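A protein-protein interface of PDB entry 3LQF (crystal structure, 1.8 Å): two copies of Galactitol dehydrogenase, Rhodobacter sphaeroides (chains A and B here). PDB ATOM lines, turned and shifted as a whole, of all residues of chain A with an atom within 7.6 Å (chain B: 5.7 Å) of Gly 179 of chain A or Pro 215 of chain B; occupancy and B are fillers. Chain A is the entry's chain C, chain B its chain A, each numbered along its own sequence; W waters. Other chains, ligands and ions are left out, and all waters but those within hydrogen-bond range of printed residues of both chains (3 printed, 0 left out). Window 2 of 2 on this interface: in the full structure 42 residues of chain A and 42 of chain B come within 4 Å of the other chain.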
ATOM      1  N   GLY A 135      -7.317  16.336  13.367  1.00  0.00           N
ATOM      2  CA  GLY A 135      -5.983  16.823  13.680  1.00  0.00           C
ATOM      3  C   GLY A 135      -5.481  17.817  12.638  1.00  0.00           C
ATOM      4  O   GLY A 135      -4.256  17.997  12.470  1.00  0.00           O
ATOM      5  N   ARG A 171      -7.389  33.672  20.097  1.00  0.00           N
ATOM      6  CA  ARG A 171      -6.198  33.247  20.782  1.00  0.00           C
ATOM      7  C   ARG A 171      -6.455  32.067  21.708  1.00  0.00           C
ATOM      8  O   ARG A 171      -5.645  31.143  21.763  1.00  0.00           O
ATOM      9  CB  ARG A 171      -5.591  34.457  21.510  1.00  0.00           C
ATOM     10  CG  ARG A 171      -5.013  35.441  20.439  1.00  0.00           C
ATOM     11  CD  ARG A 171      -4.853  36.862  20.959  1.00  0.00           C
ATOM     12  NE  ARG A 171      -3.857  37.028  22.029  1.00  0.00           N
ATOM     13  CZ  ARG A 171      -2.526  36.955  21.887  1.00  0.00           C
ATOM     14  NH1 ARG A 171      -1.962  36.596  20.733  1.00  0.00           N
ATOM     15  NH2 ARG A 171      -1.739  37.198  22.931  1.00  0.00           N
ATOM     16  N   LEU A 173      -8.759  29.738  21.428  1.00  0.00           N
ATOM     17  CA  LEU A 173      -8.892  28.527  20.605  1.00  0.00           C
ATOM     18  C   LEU A 173      -7.589  28.116  19.948  1.00  0.00           C
ATOM     19  O   LEU A 173      -7.332  26.904  19.799  1.00  0.00           O
ATOM     20  CB  LEU A 173      -9.993  28.705  19.562  1.00  0.00           C
ATOM     21  CG  LEU A 173     -11.431  28.865  20.105  1.00  0.00           C
ATOM     22  CD1 LEU A 173     -12.406  28.939  18.950  1.00  0.00           C
ATOM     23  CD2 LEU A 173     -11.803  27.750  21.081  1.00  0.00           C
ATOM     24  N   ALA A 174      -6.797  29.112  19.517  1.00  0.00           N
ATOM     25  CA  ALA A 174      -5.446  28.850  19.016  1.00  0.00           C
ATOM     26  C   ALA A 174      -4.674  28.012  20.020  1.00  0.00           C
ATOM     27  O   ALA A 174      -4.085  27.011  19.632  1.00  0.00           O
ATOM     28  CB  ALA A 174      -4.701  30.140  18.764  1.00  0.00           C
ATOM     29  N   ALA A 175      -4.693  28.415  21.291  1.00  0.00           N
ATOM     30  CA  ALA A 175      -3.910  27.745  22.340  1.00  0.00           C
ATOM     31  C   ALA A 175      -4.450  26.357  22.655  1.00  0.00           C
ATOM     32  O   ALA A 175      -3.671  25.401  22.812  1.00  0.00           O
ATOM     33  CB  ALA A 175      -3.877  28.582  23.597  1.00  0.00           C
ATOM     34  N   GLU A 176      -5.774  26.247  22.724  1.00  0.00           N
ATOM     35  CA  GLU A 176      -6.432  24.989  23.063  1.00  0.00           C
ATOM     36  C   GLU A 176      -6.255  23.909  21.996  1.00  0.00           C
ATOM     37  O   GLU A 176      -6.153  22.718  22.330  1.00  0.00           O
ATOM     38  CB  GLU A 176      -7.932  25.234  23.297  1.00  0.00           C
ATOM     39  CG  GLU A 176      -8.679  23.966  23.812  1.00  0.00           C
ATOM     40  CD  GLU A 176      -9.982  24.260  24.521  1.00  0.00           C
ATOM     41  OE1 GLU A 176     -10.293  25.438  24.820  1.00  0.00           O
ATOM     42  OE2 GLU A 176     -10.698  23.289  24.807  1.00  0.00           O
ATOM     43  N   TRP A 177      -6.252  24.322  20.727  1.00  0.00           N
ATOM     44  CA  TRP A 177      -6.245  23.383  19.594  1.00  0.00           C
ATOM     45  C   TRP A 177      -4.909  23.260  18.847  1.00  0.00           C
ATOM     46  O   TRP A 177      -4.771  22.393  17.974  1.00  0.00           O
ATOM     47  CB  TRP A 177      -7.369  23.717  18.598  1.00  0.00           C
ATOM     48  CG  TRP A 177      -8.779  23.544  19.154  1.00  0.00           C
ATOM     49  CD1 TRP A 177      -9.179  22.784  20.226  1.00  0.00           C
ATOM     50  CD2 TRP A 177      -9.964  24.126  18.622  1.00  0.00           C
ATOM     51  NE1 TRP A 177     -10.554  22.894  20.412  1.00  0.00           N
ATOM     52  CE2 TRP A 177     -11.049  23.705  19.419  1.00  0.00           C
ATOM     53  CE3 TRP A 177     -10.218  24.982  17.534  1.00  0.00           C
ATOM     54  CZ2 TRP A 177     -12.372  24.110  19.161  1.00  0.00           C
ATOM     55  CZ3 TRP A 177     -11.512  25.386  17.300  1.00  0.00           C
ATOM     56  CH2 TRP A 177     -12.581  24.942  18.083  1.00  0.00           C
ATOM     57  N   ALA A 178      -3.928  24.095  19.199  1.00  0.00           N
ATOM     58  CA  ALA A 178      -2.602  24.044  18.549  1.00  0.00           C
ATOM     59  C   ALA A 178      -1.993  22.637  18.525  1.00  0.00           C
ATOM     60  O   ALA A 178      -1.459  22.209  17.512  1.00  0.00           O
ATOM     61  CB  ALA A 178      -1.631  25.018  19.238  1.00  0.00           C
ATOM     62  N   GLY A 179      -2.057  21.932  19.651  1.00  0.00           N
ATOM     63  CA  GLY A 179      -1.491  20.577  19.744  1.00  0.00           C
ATOM     64  C   GLY A 179      -2.228  19.540  18.904  1.00  0.00           C
ATOM     65  O   GLY A 179      -1.703  18.436  18.658  1.00  0.00           O
ATOM     66  N   ARG A 180      -3.428  19.895  18.454  1.00  0.00           N
ATOM     67  CA  ARG A 180      -4.255  19.028  17.621  1.00  0.00           C
ATOM     68  C   ARG A 180      -4.359  19.579  16.216  1.00  0.00           C
ATOM     69  O   ARG A 180      -5.288  19.260  15.467  1.00  0.00           O
ATOM     70  CB  ARG A 180      -5.639  18.833  18.255  1.00  0.00           C
ATOM     71  CG  ARG A 180      -5.545  17.902  19.485  1.00  0.00           C
ATOM     72  CD  ARG A 180      -6.790  17.959  20.346  1.00  0.00           C
ATOM     73  NE  ARG A 180      -6.770  19.107  21.260  1.00  0.00           N
ATOM     74  CZ  ARG A 180      -7.729  19.367  22.142  1.00  0.00           C
ATOM     75  NH1 ARG A 180      -8.769  18.566  22.208  1.00  0.00           N
ATOM     76  NH2 ARG A 180      -7.647  20.428  22.953  1.00  0.00           N
ATOM     77  N   GLY A 181      -3.396  20.424  15.865  1.00  0.00           N
ATOM     78  CA  GLY A 181      -3.186  20.805  14.477  1.00  0.00           C
ATOM     79  C   GLY A 181      -4.203  21.733  13.850  1.00  0.00           C
ATOM     80  O   GLY A 181      -4.273  21.804  12.633  1.00  0.00           O
ATOM     81  N   VAL A 182      -4.988  22.435  14.668  1.00  0.00           N
ATOM     82  CA  VAL A 182      -5.926  23.428  14.136  1.00  0.00           C
ATOM     83  C   VAL A 182      -5.418  24.851  14.429  1.00  0.00           C
ATOM     84  O   VAL A 182      -5.278  25.229  15.588  1.00  0.00           O
ATOM     85  CB  VAL A 182      -7.346  23.246  14.703  1.00  0.00           C
ATOM     86  CG1 VAL A 182      -8.305  24.263  14.048  1.00  0.00           C
ATOM     87  CG2 VAL A 182      -7.856  21.773  14.497  1.00  0.00           C
ATOM     88  N   TYR A 239       2.944  28.178  10.305  1.00  0.00           N
ATOM     89  CA  TYR A 239       3.488  28.496  11.632  1.00  0.00           C
ATOM     90  C   TYR A 239       2.852  29.731  12.287  1.00  0.00           C
ATOM     91  O   TYR A 239       3.389  30.284  13.272  1.00  0.00           O
ATOM     92  CB  TYR A 239       5.021  28.643  11.594  1.00  0.00           C
ATOM     93  CG  TYR A 239       5.716  28.386  12.937  1.00  0.00           C
ATOM     94  CD1 TYR A 239       5.545  27.182  13.615  1.00  0.00           C
ATOM     95  CD2 TYR A 239       6.583  29.325  13.482  1.00  0.00           C
ATOM     96  CE1 TYR A 239       6.199  26.938  14.799  1.00  0.00           C
ATOM     97  CE2 TYR A 239       7.269  29.077  14.688  1.00  0.00           C
ATOM     98  CZ  TYR A 239       7.059  27.900  15.338  1.00  0.00           C
ATOM     99  OH  TYR A 239       7.712  27.654  16.524  1.00  0.00           O
ATOM    100  N   THR A 241      -0.369  30.963  14.273  1.00  0.00           N
ATOM    101  CA  THR A 241      -1.570  30.682  15.049  1.00  0.00           C
ATOM    102  C   THR A 241      -1.693  31.647  16.232  1.00  0.00           C
ATOM    103  O   THR A 241      -0.689  32.020  16.856  1.00  0.00           O
ATOM    104  CB  THR A 241      -1.690  29.180  15.486  1.00  0.00           C
ATOM    105  OG1 THR A 241      -3.045  28.903  15.836  1.00  0.00           O
ATOM    106  CG2 THR A 241      -0.718  28.783  16.635  1.00  0.00           C
ATOM    107  N   LEU B 211      10.294  24.394  23.454  1.00  0.00           N
ATOM    108  CA  LEU B 211       9.180  23.618  22.904  1.00  0.00           C
ATOM    109  C   LEU B 211       7.957  23.626  23.831  1.00  0.00           C
ATOM    110  O   LEU B 211       6.829  23.777  23.358  1.00  0.00           O
ATOM    111  CB  LEU B 211       9.593  22.178  22.562  1.00  0.00           C
ATOM    112  CG  LEU B 211      10.686  21.989  21.506  1.00  0.00           C
ATOM    113  CD1 LEU B 211      10.774  20.548  21.079  1.00  0.00           C
ATOM    114  CD2 LEU B 211      10.444  22.851  20.276  1.00  0.00           C
ATOM    115  N   ASP B 212       8.184  23.477  25.136  1.00  0.00           N
ATOM    116  CA  ASP B 212       7.093  23.526  26.111  1.00  0.00           C
ATOM    117  C   ASP B 212       6.378  24.896  26.182  1.00  0.00           C
ATOM    118  O   ASP B 212       5.204  24.959  26.588  1.00  0.00           O
ATOM    119  CB  ASP B 212       7.587  23.108  27.493  1.00  0.00           C
ATOM    120  CG  ASP B 212       6.475  23.076  28.515  1.00  0.00           C
ATOM    121  OD1 ASP B 212       5.626  22.163  28.439  1.00  0.00           O
ATOM    122  OD2 ASP B 212       6.435  23.987  29.372  1.00  0.00           O
ATOM    123  N   MET B 213       7.070  25.978  25.791  1.00  0.00           N
ATOM    124  CA  MET B 213       6.486  27.328  25.777  1.00  0.00           C
ATOM    125  C   MET B 213       5.820  27.657  24.441  1.00  0.00           C
ATOM    126  O   MET B 213       5.265  28.753  24.273  1.00  0.00           O
ATOM    127  CB  MET B 213       7.562  28.385  26.060  1.00  0.00           C
ATOM    128  CG  MET B 213       8.192  28.333  27.428  1.00  0.00           C
ATOM    129  SD  MET B 213       7.175  28.964  28.757  1.00  0.00           S
ATOM    130  CE  MET B 213       7.985  27.994  30.042  1.00  0.00           C
ATOM    131  N   THR B 214       5.910  26.733  23.481  1.00  0.00           N
ATOM    132  CA  THR B 214       5.360  26.934  22.131  1.00  0.00           C
ATOM    133  C   THR B 214       4.142  26.026  21.971  1.00  0.00           C
ATOM    134  O   THR B 214       4.274  24.817  22.096  1.00  0.00           O
ATOM    135  CB  THR B 214       6.423  26.586  21.039  1.00  0.00           C
ATOM    136  OG1 THR B 214       7.568  27.422  21.220  1.00  0.00           O
ATOM    137  CG2 THR B 214       5.859  26.778  19.646  1.00  0.00           C
ATOM    138  N   PRO B 215       2.944  26.603  21.761  1.00  0.00           N
ATOM    139  CA  PRO B 215       1.735  25.777  21.670  1.00  0.00           C
ATOM    140  C   PRO B 215       1.800  24.725  20.554  1.00  0.00           C
ATOM    141  O   PRO B 215       1.305  23.607  20.747  1.00  0.00           O
ATOM    142  CB  PRO B 215       0.619  26.812  21.407  1.00  0.00           C
ATOM    143  CG  PRO B 215       1.089  28.037  22.164  1.00  0.00           C
ATOM    144  CD  PRO B 215       2.621  28.034  21.935  1.00  0.00           C
ATOM    145  N   MET B 216       2.427  25.048  19.416  1.00  0.00           N
ATOM    146  CA  MET B 216       2.617  24.053  18.350  1.00  0.00           C
ATOM    147  C   MET B 216       3.663  22.962  18.703  1.00  0.00           C
ATOM    148  O   MET B 216       3.741  21.908  18.028  1.00  0.00           O
ATOM    149  CB  MET B 216       2.955  24.717  17.010  1.00  0.00           C
ATOM    150  CG  MET B 216       1.814  25.509  16.369  1.00  0.00           C
ATOM    151  SD  MET B 216       2.175  25.772  14.631  1.00  0.00           S
ATOM    152  CE  MET B 216       2.246  24.052  14.134  1.00  0.00           C
ATOM    153  N   GLY B 217       4.443  23.196  19.757  1.00  0.00           N
ATOM    154  CA  GLY B 217       5.421  22.182  20.223  1.00  0.00           C
ATOM    155  C   GLY B 217       6.588  21.897  19.287  1.00  0.00           C
ATOM    156  O   GLY B 217       7.186  20.803  19.335  1.00  0.00           O
ATOM    157  N   ASP B 248       4.940  32.506  15.151  1.00  0.00           N
ATOM    158  CA  ASP B 248       5.631  31.938  16.319  1.00  0.00           C
ATOM    159  C   ASP B 248       5.018  30.667  16.905  1.00  0.00           C
ATOM    160  O   ASP B 248       5.303  30.309  18.065  1.00  0.00           O
ATOM    161  CB  ASP B 248       5.758  33.017  17.393  1.00  0.00           C
ATOM    162  CG  ASP B 248       4.413  33.436  17.964  1.00  0.00           C
ATOM    163  OD1 ASP B 248       3.368  32.846  17.615  1.00  0.00           O
ATOM    164  OD2 ASP B 248       4.420  34.388  18.751  1.00  0.00           O
ATOM    165  N   GLY B 249       4.232  29.946  16.101  1.00  0.00           N
ATOM    166  CA  GLY B 249       3.563  28.700  16.561  1.00  0.00           C
ATOM    167  C   GLY B 249       2.695  28.905  17.816  1.00  0.00           C
ATOM    168  O   GLY B 249       2.430  27.940  18.578  1.00  0.00           O
ATOM    169  N   GLY B 250       2.293  30.157  18.053  1.00  0.00           N
ATOM    170  CA  GLY B 250       1.456  30.545  19.192  1.00  0.00           C
ATOM    171  C   GLY B 250       2.237  30.967  20.426  1.00  0.00           C
ATOM    172  O   GLY B 250       1.628  31.213  21.461  1.00  0.00           O
ATOM    173  N   TYR B 251       3.572  31.024  20.341  1.00  0.00           N
ATOM    174  CA  TYR B 251       4.390  31.436  21.501  1.00  0.00           C
ATOM    175  C   TYR B 251       3.878  32.657  22.287  1.00  0.00           C
ATOM    176  O   TYR B 251       3.784  32.611  23.515  1.00  0.00           O
ATOM    177  CB  TYR B 251       5.865  31.635  21.138  1.00  0.00           C
ATOM    178  CG  TYR B 251       6.798  31.596  22.342  1.00  0.00           C
ATOM    179  CD1 TYR B 251       6.893  32.684  23.200  1.00  0.00           C
ATOM    180  CD2 TYR B 251       7.627  30.489  22.569  1.00  0.00           C
ATOM    181  CE1 TYR B 251       7.768  32.674  24.290  1.00  0.00           C
ATOM    182  CE2 TYR B 251       8.500  30.460  23.635  1.00  0.00           C
ATOM    183  CZ  TYR B 251       8.569  31.556  24.497  1.00  0.00           C
ATOM    184  OH  TYR B 251       9.438  31.542  25.566  1.00  0.00           O
ATOM    185  N   VAL B 253       0.936  33.791  22.484  1.00  0.00           N
ATOM    186  CA  VAL B 253      -0.458  33.619  22.918  1.00  0.00           C
ATOM    187  C   VAL B 253      -0.544  33.319  24.417  1.00  0.00           C
ATOM    188  O   VAL B 253      -1.438  33.813  25.104  1.00  0.00           O
ATOM    189  CB  VAL B 253      -1.151  32.477  22.125  1.00  0.00           C
ATOM    190  CG1 VAL B 253      -2.533  32.159  22.685  1.00  0.00           C
ATOM    191  CG2 VAL B 253      -1.250  32.853  20.627  1.00  0.00           C
ATOM    192  N   TRP B 254       0.320  32.425  24.884  1.00  0.00           N
ATOM    193  CA  TRP B 254       0.416  32.130  26.320  1.00  0.00           C
ATOM    194  C   TRP B 254       1.143  33.206  27.118  1.00  0.00           C
ATOM    195  O   TRP B 254       1.003  33.306  28.378  1.00  0.00           O
ATOM    196  CB  TRP B 254       1.179  30.836  26.537  1.00  0.00           C
ATOM    197  CG  TRP B 254       0.424  29.588  26.287  1.00  0.00           C
ATOM    198  CD1 TRP B 254      -0.920  29.391  26.427  1.00  0.00           C
ATOM    199  CD2 TRP B 254       0.980  28.330  25.897  1.00  0.00           C
ATOM    200  NE1 TRP B 254      -1.239  28.077  26.146  1.00  0.00           N
ATOM    201  CE2 TRP B 254      -0.090  27.402  25.831  1.00  0.00           C
ATOM    202  CE3 TRP B 254       2.288  27.879  25.652  1.00  0.00           C
ATOM    203  CZ2 TRP B 254       0.103  26.047  25.504  1.00  0.00           C
ATOM    204  CZ3 TRP B 254       2.472  26.525  25.304  1.00  0.00           C
ATOM    205  CH2 TRP B 254       1.381  25.640  25.229  1.00  0.00           C
ATOM    206  OXT TRP B 254       1.971  33.973  26.577  1.00  0.00           O
HETATM  207  O   HOH W   1       8.692  29.150  18.836  1.00  0.00           O
HETATM  208  O   HOH W   2       1.928  33.060  14.998  1.00  0.00           O
HETATM  209  O   HOH W   3       0.809  34.135  17.655  1.00  0.00           O
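N of Asp 248 of chain B lies within hydrogen-bond range of O of Tyr 239 of chain A (3.3 Å).
The backbone carbonyl oxygen of Tyr 239 of chain A sits at hydrogen-bond distance from the backbone NH of Gly 249 of chain B.
N of Met 216 of chain B sits at hydrogen-bond distance from O of Gly 249 of chain B, at 3.0 Å.
OD1 of Asp 248 of chain B sits at hydrogen-bond distance from N of Tyr 251 of chain B (3.3 Å).
The backbone NH (N) of Gly 250 of chain B sits at hydrogen-bond distance from the side-chain carboxylate (OD1) of Asp 248 of chain B (2.9 Å).
Val 253 of chain B touches Arg 171 of chain A.
Val 253 of chain B touches Ala 175 of chain A (CG1 to CB, 3.9 Å).
Ala 175 of chain A touches Trp 254 of chain B.
O of Pro 215 of chain B touches CB of Ala 178 of chain A, 3.6 Å away.
N of Gly 179 of chain A touches O of Pro 215 of chain B (3.9 Å).
OH of Tyr 239 of chain A touches CG2 of Thr 214 of chain B, 3.7 Å away.
CD1 of Tyr 239 of chain A touches SD of Met 216 of chain B, 3.8 Å away.
Thr 241 of chain A touches Gly 249 of chain B.
Thr 241 of chain A touches Gly 250 of chain B (O to CA, 3.5 Å).
Val 253 of chain B touches Thr 241 of chain A (CG2 to O, 3.9 Å).
Printed residues of chain B within 4 Å of Ala 178 of chain A: Pro 215.
Gly 179 of chain A touches just one residue of chain B: Pro 215 (3.9 Å).
Printed residues of chain A within 4 Å of Thr 214 of chain B: Tyr 239.
Pro 215 of chain B touches just these residues of chain A: Ala 178 and Gly 179.
The nearest printed residue of chain B that does not touch Gly 179 of chain A is Met 216 of chain B (5.3 Å).
The nearest printed residue of chain A that does not touch Asp 248 of chain B is Thr 241 of chain A (4.2 Å).
Printed residues of chain B that touch a printed residue of chain A: Thr 214, Pro 215, Met 216, Asp 248, Gly 249, Gly 250, Val 253 and Trp 254.
Hydrophobic or aromatic side chains of chain B within 4 Å of the printed part of chain A: Pro 215, Met 216, Val 253 and Trp 254.
Along chain B the printed residues that touch a printed residue of chain A span positions 214 to 254.
Hydrophobic or aromatic side chains of chain A within 4 Å of the printed part of chain B: Ala 175, Ala 178 and Tyr 239.
Among the printed residues, 12 pairs touch across the chains.
Among the printed residues, no Asp or Glu carboxylate lies within 4 Å of a Lys or Arg side-chain nitrogen of the other chain.
No position is printed for both chains.
Water W3 lies within hydrogen-bond range of the backbone carbonyl oxygen (O) of Thr 241 of chain A (2.7 Å) and the side-chain carboxylate (OD1) of Asp 248 of chain B (2.9 Å).
Water W1 lies within hydrogen-bond range of OH of Tyr 239 of chain A (2.9 Å) and OG1 of Thr 214 of chain B (3.2 Å).
Water W2 lies within hydrogen-bond range of the side-chain carboxylate of Asp 248 of chain B (3.0 Å) and the backbone NH of Thr 241 of chain A (3.2 Å).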
